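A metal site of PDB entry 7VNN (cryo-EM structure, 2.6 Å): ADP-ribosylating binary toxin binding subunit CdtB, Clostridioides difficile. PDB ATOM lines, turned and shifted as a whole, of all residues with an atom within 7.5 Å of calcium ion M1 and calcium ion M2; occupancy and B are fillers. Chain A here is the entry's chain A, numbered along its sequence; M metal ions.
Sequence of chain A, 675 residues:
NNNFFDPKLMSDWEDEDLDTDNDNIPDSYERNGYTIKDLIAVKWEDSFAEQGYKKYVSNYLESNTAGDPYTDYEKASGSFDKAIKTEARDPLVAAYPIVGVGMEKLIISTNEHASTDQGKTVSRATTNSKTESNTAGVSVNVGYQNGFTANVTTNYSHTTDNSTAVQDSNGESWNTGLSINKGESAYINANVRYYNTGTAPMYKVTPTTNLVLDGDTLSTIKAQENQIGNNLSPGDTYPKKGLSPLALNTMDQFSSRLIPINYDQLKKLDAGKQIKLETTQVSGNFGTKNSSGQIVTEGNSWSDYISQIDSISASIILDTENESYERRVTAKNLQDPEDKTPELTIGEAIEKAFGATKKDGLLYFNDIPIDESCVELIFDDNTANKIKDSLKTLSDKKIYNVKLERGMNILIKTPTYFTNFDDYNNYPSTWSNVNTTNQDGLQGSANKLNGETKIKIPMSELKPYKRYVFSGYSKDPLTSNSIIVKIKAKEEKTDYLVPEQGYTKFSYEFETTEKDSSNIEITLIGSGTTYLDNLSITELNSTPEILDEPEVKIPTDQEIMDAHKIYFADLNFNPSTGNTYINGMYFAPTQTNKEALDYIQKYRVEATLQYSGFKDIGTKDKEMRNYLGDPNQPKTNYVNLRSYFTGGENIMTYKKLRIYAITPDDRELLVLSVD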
ATOM      1  N   LEU A  18     -33.386  29.435 -17.119  1.00  0.00           N
ATOM      2  CA  LEU A  18     -32.062  29.753 -17.638  1.00  0.00           C
ATOM      3  C   LEU A  18     -31.377  28.490 -18.127  1.00  0.00           C
ATOM      4  O   LEU A  18     -31.376  27.461 -17.454  1.00  0.00           O
ATOM      5  CB  LEU A  18     -31.220  30.430 -16.550  1.00  0.00           C
ATOM      6  CG  LEU A  18     -29.967  31.162 -17.047  1.00  0.00           C
ATOM      7  CD1 LEU A  18     -30.266  31.973 -18.296  1.00  0.00           C
ATOM      8  CD2 LEU A  18     -29.413  32.051 -15.945  1.00  0.00           C
ATOM      9  N   ASP A  19     -30.777  28.586 -19.317  1.00  0.00           N
ATOM     10  CA  ASP A  19     -30.104  27.438 -19.947  1.00  0.00           C
ATOM     11  C   ASP A  19     -28.920  27.989 -20.727  1.00  0.00           C
ATOM     12  O   ASP A  19     -29.090  28.462 -21.857  1.00  0.00           O
ATOM     13  CB  ASP A  19     -31.067  26.670 -20.838  1.00  0.00           C
ATOM     14  CG  ASP A  19     -30.626  25.227 -21.048  1.00  0.00           C
ATOM     15  OD1 ASP A  19     -29.508  24.875 -20.641  1.00  0.00           O
ATOM     16  OD2 ASP A  19     -31.415  24.452 -21.634  1.00  0.00           O
ATOM     17  N   THR A  20     -27.731  27.919 -20.129  1.00  0.00           N
ATOM     18  CA  THR A  20     -26.546  28.524 -20.733  1.00  0.00           C
ATOM     19  C   THR A  20     -25.869  27.637 -21.765  1.00  0.00           C
ATOM     20  O   THR A  20     -25.438  28.130 -22.804  1.00  0.00           O
ATOM     21  CB  THR A  20     -25.541  28.901 -19.639  1.00  0.00           C
ATOM     22  OG1 THR A  20     -26.197  29.668 -18.624  1.00  0.00           O
ATOM     23  CG2 THR A  20     -24.407  29.723 -20.218  1.00  0.00           C
ATOM     24  N   ASP A  21     -25.769  26.327 -21.502  1.00  0.00           N
ATOM     25  CA  ASP A  21     -25.146  25.415 -22.438  1.00  0.00           C
ATOM     26  C   ASP A  21     -26.110  24.883 -23.503  1.00  0.00           C
ATOM     27  O   ASP A  21     -25.661  24.215 -24.432  1.00  0.00           O
ATOM     28  CB  ASP A  21     -24.521  24.232 -21.691  1.00  0.00           C
ATOM     29  CG  ASP A  21     -25.482  23.591 -20.711  1.00  0.00           C
ATOM     30  OD1 ASP A  21     -26.644  24.042 -20.631  1.00  0.00           O
ATOM     31  OD2 ASP A  21     -25.081  22.643 -20.007  1.00  0.00           O
ATOM     32  N   ASN A  22     -27.400  25.174 -23.370  1.00  0.00           N
ATOM     33  CA  ASN A  22     -28.429  24.766 -24.334  1.00  0.00           C
ATOM     34  C   ASN A  22     -28.463  23.247 -24.493  1.00  0.00           C
ATOM     35  O   ASN A  22     -28.301  22.708 -25.584  1.00  0.00           O
ATOM     36  CB  ASN A  22     -28.202  25.457 -25.680  1.00  0.00           C
ATOM     37  CG  ASN A  22     -28.938  26.784 -25.776  1.00  0.00           C
ATOM     38  OD1 ASN A  22     -29.143  27.464 -24.777  1.00  0.00           O
ATOM     39  ND2 ASN A  22     -29.330  27.152 -26.984  1.00  0.00           N
ATOM     40  N   ASP A  23     -28.698  22.552 -23.373  1.00  0.00           N
ATOM     41  CA  ASP A  23     -28.951  21.117 -23.380  1.00  0.00           C
ATOM     42  C   ASP A  23     -30.334  20.776 -22.836  1.00  0.00           C
ATOM     43  O   ASP A  23     -30.551  19.674 -22.333  1.00  0.00           O
ATOM     44  CB  ASP A  23     -27.862  20.383 -22.596  1.00  0.00           C
ATOM     45  CG  ASP A  23     -27.757  20.838 -21.162  1.00  0.00           C
ATOM     46  OD1 ASP A  23     -28.445  21.805 -20.778  1.00  0.00           O
ATOM     47  OD2 ASP A  23     -26.984  20.224 -20.398  1.00  0.00           O
ATOM     48  N   ASN A  24     -31.274  21.716 -22.913  1.00  0.00           N
ATOM     49  CA  ASN A  24     -32.675  21.561 -22.528  1.00  0.00           C
ATOM     50  C   ASN A  24     -32.870  21.343 -21.031  1.00  0.00           C
ATOM     51  O   ASN A  24     -33.998  21.089 -20.594  1.00  0.00           O
ATOM     52  CB  ASN A  24     -33.362  20.430 -23.298  1.00  0.00           C
ATOM     53  CG  ASN A  24     -32.936  20.378 -24.753  1.00  0.00           C
ATOM     54  OD1 ASN A  24     -32.896  21.394 -25.438  1.00  0.00           O
ATOM     55  ND2 ASN A  24     -32.629  19.176 -25.226  1.00  0.00           N
ATOM     56  N   ILE A  25     -31.809  21.436 -20.233  1.00  0.00           N
ATOM     57  CA  ILE A  25     -31.894  21.299 -18.785  1.00  0.00           C
ATOM     58  C   ILE A  25     -31.561  22.650 -18.169  1.00  0.00           C
ATOM     59  O   ILE A  25     -30.499  23.204 -18.462  1.00  0.00           O
ATOM     60  CB  ILE A  25     -30.951  20.218 -18.234  1.00  0.00           C
ATOM     61  CG1 ILE A  25     -31.075  18.933 -19.050  1.00  0.00           C
ATOM     62  CG2 ILE A  25     -31.263  19.934 -16.770  1.00  0.00           C
ATOM     63  CD1 ILE A  25     -29.991  17.923 -18.763  1.00  0.00           C
ATOM     64  N   PRO A  26     -32.428  23.224 -17.338  1.00  0.00           N
ATOM     65  CA  PRO A  26     -32.111  24.510 -16.707  1.00  0.00           C
ATOM     66  C   PRO A  26     -30.898  24.421 -15.795  1.00  0.00           C
ATOM     67  O   PRO A  26     -30.580  23.360 -15.256  1.00  0.00           O
ATOM     68  CB  PRO A  26     -33.384  24.841 -15.917  1.00  0.00           C
ATOM     69  CG  PRO A  26     -34.458  24.081 -16.614  1.00  0.00           C
ATOM     70  CD  PRO A  26     -33.824  22.824 -17.100  1.00  0.00           C
ATOM     71  N   ASP A  27     -30.212  25.561 -15.645  1.00  0.00           N
ATOM     72  CA  ASP A  27     -28.969  25.602 -14.884  1.00  0.00           C
ATOM     73  C   ASP A  27     -29.191  25.235 -13.423  1.00  0.00           C
ATOM     74  O   ASP A  27     -28.387  24.497 -12.833  1.00  0.00           O
ATOM     75  CB  ASP A  27     -28.344  26.985 -14.994  1.00  0.00           C
ATOM     76  CG  ASP A  27     -27.902  27.314 -16.399  1.00  0.00           C
ATOM     77  OD1 ASP A  27     -28.083  26.460 -17.300  1.00  0.00           O
ATOM     78  OD2 ASP A  27     -27.364  28.421 -16.624  1.00  0.00           O
ATOM     79  N   SER A  28     -30.262  25.751 -12.818  1.00  0.00           N
ATOM     80  CA  SER A  28     -30.513  25.469 -11.401  1.00  0.00           C
ATOM     81  C   SER A  28     -30.777  23.987 -11.179  1.00  0.00           C
ATOM     82  O   SER A  28     -30.389  23.430 -10.148  1.00  0.00           O
ATOM     83  CB  SER A  28     -31.663  26.323 -10.897  1.00  0.00           C
ATOM     84  OG  SER A  28     -32.801  26.208 -11.738  1.00  0.00           O
ATOM     85  N   GLU A  30     -29.453  21.550 -12.961  1.00  0.00           N
ATOM     86  CA  GLU A  30     -28.155  20.899 -13.078  1.00  0.00           C
ATOM     87  C   GLU A  30     -27.334  21.099 -11.813  1.00  0.00           C
ATOM     88  O   GLU A  30     -26.574  20.207 -11.409  1.00  0.00           O
ATOM     89  CB  GLU A  30     -27.399  21.438 -14.295  1.00  0.00           C
ATOM     90  CG  GLU A  30     -28.066  21.137 -15.622  1.00  0.00           C
ATOM     91  CD  GLU A  30     -27.069  21.101 -16.761  1.00  0.00           C
ATOM     92  OE1 GLU A  30     -26.178  20.233 -16.753  1.00  0.00           O
ATOM     93  OE2 GLU A  30     -27.179  21.940 -17.677  1.00  0.00           O
ATOM     94  N   TYR A  34     -31.677  16.732 -10.539  1.00  0.00           N
ATOM     95  CA  TYR A  34     -32.883  16.629 -11.361  1.00  0.00           C
ATOM     96  C   TYR A  34     -33.086  15.172 -11.744  1.00  0.00           C
ATOM     97  O   TYR A  34     -32.298  14.296 -11.399  1.00  0.00           O
ATOM     98  CB  TYR A  34     -32.765  17.514 -12.604  1.00  0.00           C
ATOM     99  CG  TYR A  34     -31.628  17.153 -13.525  1.00  0.00           C
ATOM    100  CD1 TYR A  34     -30.344  17.599 -13.288  1.00  0.00           C
ATOM    101  CD2 TYR A  34     -31.838  16.344 -14.644  1.00  0.00           C
ATOM    102  CE1 TYR A  34     -29.294  17.271 -14.123  1.00  0.00           C
ATOM    103  CE2 TYR A  34     -30.805  16.000 -15.486  1.00  0.00           C
ATOM    104  CZ  TYR A  34     -29.534  16.467 -15.214  1.00  0.00           C
ATOM    105  OH  TYR A  34     -28.494  16.145 -16.057  1.00  0.00           O
ATOM    106  N   SER A  58     -24.877  17.805 -13.051  1.00  0.00           N
ATOM    107  CA  SER A  58     -23.990  17.951 -14.201  1.00  0.00           C
ATOM    108  C   SER A  58     -23.515  19.393 -14.293  1.00  0.00           C
ATOM    109  O   SER A  58     -24.044  20.290 -13.641  1.00  0.00           O
ATOM    110  CB  SER A  58     -24.703  17.521 -15.497  1.00  0.00           C
ATOM    111  OG  SER A  58     -25.981  18.119 -15.592  1.00  0.00           O
ATOM    112  N   ASN A  59     -22.496  19.587 -15.126  1.00  0.00           N
ATOM    113  CA  ASN A  59     -21.972  20.914 -15.407  1.00  0.00           C
ATOM    114  C   ASN A  59     -22.980  21.706 -16.212  1.00  0.00           C
ATOM    115  O   ASN A  59     -23.410  21.273 -17.292  1.00  0.00           O
ATOM    116  CB  ASN A  59     -20.644  20.789 -16.159  1.00  0.00           C
ATOM    117  CG  ASN A  59     -19.900  22.104 -16.270  1.00  0.00           C
ATOM    118  OD1 ASN A  59     -20.464  23.176 -16.072  1.00  0.00           O
ATOM    119  ND2 ASN A  59     -18.620  22.028 -16.584  1.00  0.00           N
ATOM    120  N   TYR A  60     -23.366  22.878 -15.709  1.00  0.00           N
ATOM    121  CA  TYR A  60     -24.365  23.711 -16.361  1.00  0.00           C
ATOM    122  C   TYR A  60     -23.782  24.640 -17.415  1.00  0.00           C
ATOM    123  O   TYR A  60     -24.542  25.310 -18.121  1.00  0.00           O
ATOM    124  CB  TYR A  60     -25.148  24.531 -15.323  1.00  0.00           C
ATOM    125  CG  TYR A  60     -24.349  25.653 -14.685  1.00  0.00           C
ATOM    126  CD1 TYR A  60     -23.518  25.403 -13.602  1.00  0.00           C
ATOM    127  CD2 TYR A  60     -24.458  26.952 -15.152  1.00  0.00           C
ATOM    128  CE1 TYR A  60     -22.803  26.424 -13.016  1.00  0.00           C
ATOM    129  CE2 TYR A  60     -23.736  27.980 -14.568  1.00  0.00           C
ATOM    130  CZ  TYR A  60     -22.909  27.702 -13.504  1.00  0.00           C
ATOM    131  OH  TYR A  60     -22.194  28.723 -12.918  1.00  0.00           O
ATOM    132  N   LEU A  61     -22.455  24.703 -17.534  1.00  0.00           N
ATOM    133  CA  LEU A  61     -21.798  25.499 -18.568  1.00  0.00           C
ATOM    134  C   LEU A  61     -21.285  24.652 -19.722  1.00  0.00           C
ATOM    135  O   LEU A  61     -20.704  25.197 -20.655  1.00  0.00           O
ATOM    136  CB  LEU A  61     -20.650  26.319 -17.972  1.00  0.00           C
ATOM    137  CG  LEU A  61     -21.032  27.506 -17.087  1.00  0.00           C
ATOM    138  CD1 LEU A  61     -19.781  28.231 -16.612  1.00  0.00           C
ATOM    139  CD2 LEU A  61     -21.948  28.449 -17.832  1.00  0.00           C
ATOM    140  N   GLU A  62     -21.482  23.331 -19.671  1.00  0.00           N
ATOM    141  CA  GLU A  62     -21.050  22.431 -20.721  1.00  0.00           C
ATOM    142  C   GLU A  62     -22.172  21.467 -21.067  1.00  0.00           C
ATOM    143  O   GLU A  62     -22.827  20.927 -20.166  1.00  0.00           O
ATOM    144  CB  GLU A  62     -19.798  21.643 -20.300  1.00  0.00           C
ATOM    145  CG  GLU A  62     -18.888  21.259 -21.451  1.00  0.00           C
ATOM    146  CD  GLU A  62     -17.695  20.433 -21.005  1.00  0.00           C
ATOM    147  OE1 GLU A  62     -17.366  20.466 -19.798  1.00  0.00           O
ATOM    148  OE2 GLU A  62     -17.107  19.739 -21.857  1.00  0.00           O
ATOM    149  N   SER A  63     -22.402  21.268 -22.362  1.00  0.00           N
ATOM    150  CA  SER A  63     -23.409  20.315 -22.799  1.00  0.00           C
ATOM    151  C   SER A  63     -22.959  18.867 -22.691  1.00  0.00           C
ATOM    152  O   SER A  63     -23.797  17.968 -22.645  1.00  0.00           O
ATOM    153  CB  SER A  63     -23.817  20.616 -24.241  1.00  0.00           C
ATOM    154  OG  SER A  63     -24.853  19.747 -24.669  1.00  0.00           O
ATOM    155  N   ASN A  64     -21.645  18.624 -22.644  1.00  0.00           N
ATOM    156  CA  ASN A  64     -21.068  17.286 -22.516  1.00  0.00           C
ATOM    157  C   ASN A  64     -20.187  17.290 -21.268  1.00  0.00           C
ATOM    158  O   ASN A  64     -18.996  17.611 -21.349  1.00  0.00           O
ATOM    159  CB  ASN A  64     -20.294  16.893 -23.766  1.00  0.00           C
ATOM    160  CG  ASN A  64     -21.187  16.612 -24.951  1.00  0.00           C
ATOM    161  OD1 ASN A  64     -21.563  15.481 -25.203  1.00  0.00           O
ATOM    162  ND2 ASN A  64     -21.548  17.667 -25.685  1.00  0.00           N
ATOM    163  N   THR A  65     -20.777  16.953 -20.124  1.00  0.00           N
ATOM    164  CA  THR A  65     -20.028  16.982 -18.873  1.00  0.00           C
ATOM    165  C   THR A  65     -18.912  15.935 -18.863  1.00  0.00           C
ATOM    166  O   THR A  65     -17.791  16.219 -18.430  1.00  0.00           O
ATOM    167  CB  THR A  65     -20.969  16.757 -17.688  1.00  0.00           C
ATOM    168  OG1 THR A  65     -22.053  17.692 -17.759  1.00  0.00           O
ATOM    169  CG2 THR A  65     -20.238  16.940 -16.379  1.00  0.00           C
ATOM    170  N   THR A  71     -24.767  14.118 -25.110  1.00  0.00           N
ATOM    171  CA  THR A  71     -25.005  15.252 -24.243  1.00  0.00           C
ATOM    172  C   THR A  71     -25.616  14.799 -22.909  1.00  0.00           C
ATOM    173  O   THR A  71     -26.004  13.641 -22.734  1.00  0.00           O
ATOM    174  CB  THR A  71     -25.920  16.279 -24.915  1.00  0.00           C
ATOM    175  OG1 THR A  71     -27.275  15.833 -24.834  1.00  0.00           O
ATOM    176  CG2 THR A  71     -25.539  16.445 -26.378  1.00  0.00           C
ATOM    177  N   ASP A  72     -25.699  15.752 -21.970  1.00  0.00           N
ATOM    178  CA  ASP A  72     -26.205  15.437 -20.641  1.00  0.00           C
ATOM    179  C   ASP A  72     -27.673  15.011 -20.684  1.00  0.00           C
ATOM    180  O   ASP A  72     -28.067  14.036 -20.032  1.00  0.00           O
ATOM    181  CB  ASP A  72     -26.021  16.637 -19.718  1.00  0.00           C
ATOM    182  CG  ASP A  72     -24.566  16.925 -19.434  1.00  0.00           C
ATOM    183  OD1 ASP A  72     -23.728  16.029 -19.630  1.00  0.00           O
ATOM    184  OD2 ASP A  72     -24.262  18.065 -19.008  1.00  0.00           O
ATOM    185  N   TYR A  73     -28.498  15.744 -21.435  1.00  0.00           N
ATOM    186  CA  TYR A  73     -29.910  15.391 -21.534  1.00  0.00           C
ATOM    187  C   TYR A  73     -30.093  14.039 -22.220  1.00  0.00           C
ATOM    188  O   TYR A  73     -30.935  13.240 -21.810  1.00  0.00           O
ATOM    189  CB  TYR A  73     -30.690  16.472 -22.272  1.00  0.00           C
ATOM    190  CG  TYR A  73     -32.128  16.093 -22.530  1.00  0.00           C
ATOM    191  CD1 TYR A  73     -33.071  16.132 -21.518  1.00  0.00           C
ATOM    192  CD2 TYR A  73     -32.540  15.684 -23.790  1.00  0.00           C
ATOM    193  CE1 TYR A  73     -34.385  15.783 -21.746  1.00  0.00           C
ATOM    194  CE2 TYR A  73     -33.849  15.329 -24.029  1.00  0.00           C
ATOM    195  CZ  TYR A  73     -34.768  15.389 -23.003  1.00  0.00           C
ATOM    196  OH  TYR A  73     -36.075  15.034 -23.233  1.00  0.00           O
ATOM    197  N   PRO A  91     -24.696  11.949 -16.175  1.00  0.00           N
ATOM    198  CA  PRO A  91     -23.746  12.756 -16.954  1.00  0.00           C
ATOM    199  C   PRO A  91     -22.309  12.665 -16.473  1.00  0.00           C
ATOM    200  O   PRO A  91     -21.412  13.074 -17.220  1.00  0.00           O
ATOM    201  CB  PRO A  91     -24.302  14.183 -16.797  1.00  0.00           C
ATOM    202  CG  PRO A  91     -25.735  14.000 -16.424  1.00  0.00           C
ATOM    203  CD  PRO A  91     -25.782  12.762 -15.595  1.00  0.00           C
HETATM  204 CA    CA M   1     -28.250  23.532 -19.027  1.00  0.00          CA
HETATM  205 CA    CA M   2     -24.917  20.432 -18.983  1.00  0.00          CA
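Calcium ion M2 is bound by the backbone carbonyl oxygen of Asn 59 (2.4 Å), the side-chain carboxylate of Asp 21 (2.4 Å), the backbone carbonyl oxygen of Glu 62 (2.5 Å), the side-chain carboxylate of Asp 72 (2.5 Å), the side-chain carboxylate of Asp 23 (2.5 Å) and the side-chain carboxylate of Glu 30 (2.6 Å).
Calcium ion M2 has six donor atoms within binding distance.
Slightly farther from calcium ion M2 lies the side-chain carboxylate (OE2) of Glu 30 (3.0 Å).
Of the 25 residues printed, 6 come within 4 Å of calcium ion M2.
Calcium ion M1 is bound by OD1 of Asp 21 (2.3 Å), O of Ile 25 (2.3 Å), OE2 of Glu 30 (2.3 Å), OD1 of Asp 19 (2.4 Å) and OD1 of Asp 23 (2.5 Å).
OD1 of Asp 72 lies within hydrogen-bond range of OG1 of Thr 65 (3.0 Å).
The backbone NH of Leu 61 lies within hydrogen-bond range of the side-chain amide oxygen of Asn 59 (2.9 Å).
N of Asp 27 lies within hydrogen-bond range of O of Leu 18 (2.9 Å).
The side-chain carboxylate (OD2) of Asp 27 lies within hydrogen-bond range of the side-chain hydroxyl (OG1) of Thr 20, at 2.6 Å.
The backbone carbonyl oxygen of Glu 30 is in hydrogen-bond range of the backbone NH of Ser 58, 3.4 Å away.
O of Asp 19 lies close to OD1 of Asn 22 (3.1 Å).
OD2 of Asp 19 lies within hydrogen-bond range of N of Asn 24.
OG1 of Thr 65 is in hydrogen-bond range of N of Asn 59.
OD1 of Asp 27 touches calcium ion M1, at 3.4 Å.
Six residues have an atom within 4 Å of calcium ion M1: Asp 19, Asp 21, Asp 23, Ile 25, Asp 27 and Glu 30.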
